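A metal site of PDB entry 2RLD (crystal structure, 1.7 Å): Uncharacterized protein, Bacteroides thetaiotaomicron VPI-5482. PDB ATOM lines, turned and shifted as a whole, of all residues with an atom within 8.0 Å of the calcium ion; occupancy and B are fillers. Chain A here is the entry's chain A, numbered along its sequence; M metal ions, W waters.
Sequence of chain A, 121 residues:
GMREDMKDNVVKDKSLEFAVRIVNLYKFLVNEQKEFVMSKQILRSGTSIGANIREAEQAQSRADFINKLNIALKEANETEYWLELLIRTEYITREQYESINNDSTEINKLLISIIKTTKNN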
ATOM      1  N   ARG A   3     -20.025  11.217  15.437  1.00  0.00           N
ATOM      2  CA  ARG A   3     -20.208  11.501  14.026  1.00  0.00           C
ATOM      3  C   ARG A   3     -18.945  12.140  13.467  1.00  0.00           C
ATOM      4  O   ARG A   3     -18.351  13.002  14.118  1.00  0.00           O
ATOM      5  CB  ARG A   3     -21.380  12.453  13.809  1.00  0.00           C
ATOM      6  CG  ARG A   3     -22.742  11.806  13.979  1.00  0.00           C
ATOM      7  CD  ARG A   3     -23.817  12.868  13.906  1.00  0.00           C
ATOM      8  NE  ARG A   3     -23.857  13.500  12.589  1.00  0.00           N
ATOM      9  CZ  ARG A   3     -24.598  13.072  11.563  1.00  0.00           C
ATOM     10  NH1 ARG A   3     -25.351  11.980  11.675  1.00  0.00           N
ATOM     11  NH2 ARG A   3     -24.545  13.718  10.410  1.00  0.00           N
ATOM     12  N   GLU A   4     -18.539  11.726  12.266  1.00  0.00           N
ATOM     13  CA  GLU A   4     -17.331  12.292  11.673  1.00  0.00           C
ATOM     14  C   GLU A   4     -17.442  13.804  11.532  1.00  0.00           C
ATOM     15  O   GLU A   4     -16.480  14.536  11.783  1.00  0.00           O
ATOM     16  CB  GLU A   4     -17.044  11.711  10.284  1.00  0.00           C
ATOM     17  CG  GLU A   4     -16.993  10.207  10.152  1.00  0.00           C
ATOM     18  CD  GLU A   4     -15.931   9.547  11.012  1.00  0.00           C
ATOM     19  OE1 GLU A   4     -14.994  10.230  11.472  1.00  0.00           O
ATOM     20  OE2 GLU A   4     -16.059   8.303  11.183  1.00  0.00           O
ATOM     21  N   ASP A   5     -18.607  14.269  11.116  1.00  0.00           N
ATOM     22  CA  ASP A   5     -18.808  15.700  10.947  1.00  0.00           C
ATOM     23  C   ASP A   5     -18.821  16.521  12.240  1.00  0.00           C
ATOM     24  O   ASP A   5     -18.918  17.749  12.155  1.00  0.00           O
ATOM     25  CB  ASP A   5     -20.035  16.004  10.057  1.00  0.00           C
ATOM     26  CG  ASP A   5     -21.376  15.587  10.677  1.00  0.00           C
ATOM     27  OD1 ASP A   5     -21.436  15.184  11.867  1.00  0.00           O
ATOM     28  OD2 ASP A   5     -22.363  15.682   9.933  1.00  0.00           O
ATOM     29  N   MET A   6     -18.732  15.888  13.416  1.00  0.00           N
ATOM     30  CA  MET A   6     -18.662  16.626  14.680  1.00  0.00           C
ATOM     31  C   MET A   6     -17.252  16.696  15.250  1.00  0.00           C
ATOM     32  O   MET A   6     -16.997  17.475  16.172  1.00  0.00           O
ATOM     33  CB  MET A   6     -19.586  15.988  15.707  1.00  0.00           C
ATOM     34  CG  MET A   6     -21.059  16.173  15.379  1.00  0.00           C
ATOM     35  SD  MET A   6     -21.626  17.999  15.742  1.00  0.00           S
ATOM     36  CE  MET A   6     -21.091  18.927  14.093  1.00  0.00           C
ATOM     37  N   LYS A   7     -16.346  15.896  14.711  1.00  0.00           N
ATOM     38  CA  LYS A   7     -14.984  15.804  15.233  1.00  0.00           C
ATOM     39  C   LYS A   7     -14.212  17.112  15.134  1.00  0.00           C
ATOM     40  O   LYS A   7     -13.508  17.511  16.085  1.00  0.00           O
ATOM     41  CB  LYS A   7     -14.247  14.655  14.549  1.00  0.00           C
ATOM     42  CG  LYS A   7     -14.811  13.320  14.971  1.00  0.00           C
ATOM     43  CD  LYS A   7     -14.141  12.146  14.303  1.00  0.00           C
ATOM     44  CE  LYS A   7     -14.783  10.817  14.785  1.00  0.00           C
ATOM     45  NZ  LYS A   7     -14.213   9.626  14.060  1.00  0.00           N
ATOM     46  N   ASP A   8     -14.391  17.843  14.039  1.00  0.00           N
ATOM     47  CA  ASP A   8     -13.766  19.157  13.932  1.00  0.00           C
ATOM     48  C   ASP A   8     -14.331  20.158  14.957  1.00  0.00           C
ATOM     49  O   ASP A   8     -13.583  20.881  15.605  1.00  0.00           O
ATOM     50  CB  ASP A   8     -13.898  19.687  12.506  1.00  0.00           C
ATOM     51  CG  ASP A   8     -15.328  19.843  12.056  1.00  0.00           C
ATOM     52  OD1 ASP A   8     -16.203  19.041  12.471  1.00  0.00           O
ATOM     53  OD2 ASP A   8     -15.582  20.754  11.271  1.00  0.00           O
ATOM     54  N   ASN A   9     -15.652  20.160  15.116  1.00  0.00           N
ATOM     55  CA  ASN A   9     -16.296  21.029  16.099  1.00  0.00           C
ATOM     56  C   ASN A   9     -15.800  20.748  17.520  1.00  0.00           C
ATOM     57  O   ASN A   9     -15.550  21.670  18.293  1.00  0.00           O
ATOM     58  CB  ASN A   9     -17.827  20.858  16.089  1.00  0.00           C
ATOM     59  CG  ASN A   9     -18.426  20.992  14.703  1.00  0.00           C
ATOM     60  OD1 ASN A   9     -18.126  20.197  13.825  1.00  0.00           O
ATOM     61  ND2 ASN A   9     -19.281  22.000  14.505  1.00  0.00           N
ATOM     62  N   VAL A  10     -15.682  19.464  17.857  1.00  0.00           N
ATOM     63  CA  VAL A  10     -15.290  19.035  19.202  1.00  0.00           C
ATOM     64  C   VAL A  10     -13.802  19.314  19.455  1.00  0.00           C
ATOM     65  O   VAL A  10     -13.434  19.760  20.525  1.00  0.00           O
ATOM     66  CB  VAL A  10     -15.644  17.530  19.444  1.00  0.00           C
ATOM     67  CG1 VAL A  10     -15.036  17.003  20.760  1.00  0.00           C
ATOM     68  CG2 VAL A  10     -17.142  17.345  19.434  1.00  0.00           C
HETATM   69 CA    CA M   1     -18.141  19.820  11.407  1.00  0.00          CA
HETATM   70  O   HOH W   1     -17.485  22.587  10.790  1.00  0.00           O
HETATM   71  O   HOH W   2     -19.316  19.795   9.168  1.00  0.00           O
HETATM   72  O   HOH W   3     -16.976  18.603   9.555  1.00  0.00           O
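The guanidinium group (NH2) of Arg 3 is in salt-bridge range of the side-chain carboxylate (OD2) of Asp 5.
The calcium ion is bound by O of Asp 5, OD1 of Asp 8, OD1 of Asn 9, water W3, water W2 and OD2 of Asp 8. Slightly farther from the calcium ion lies water W1 (2.9 Å).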
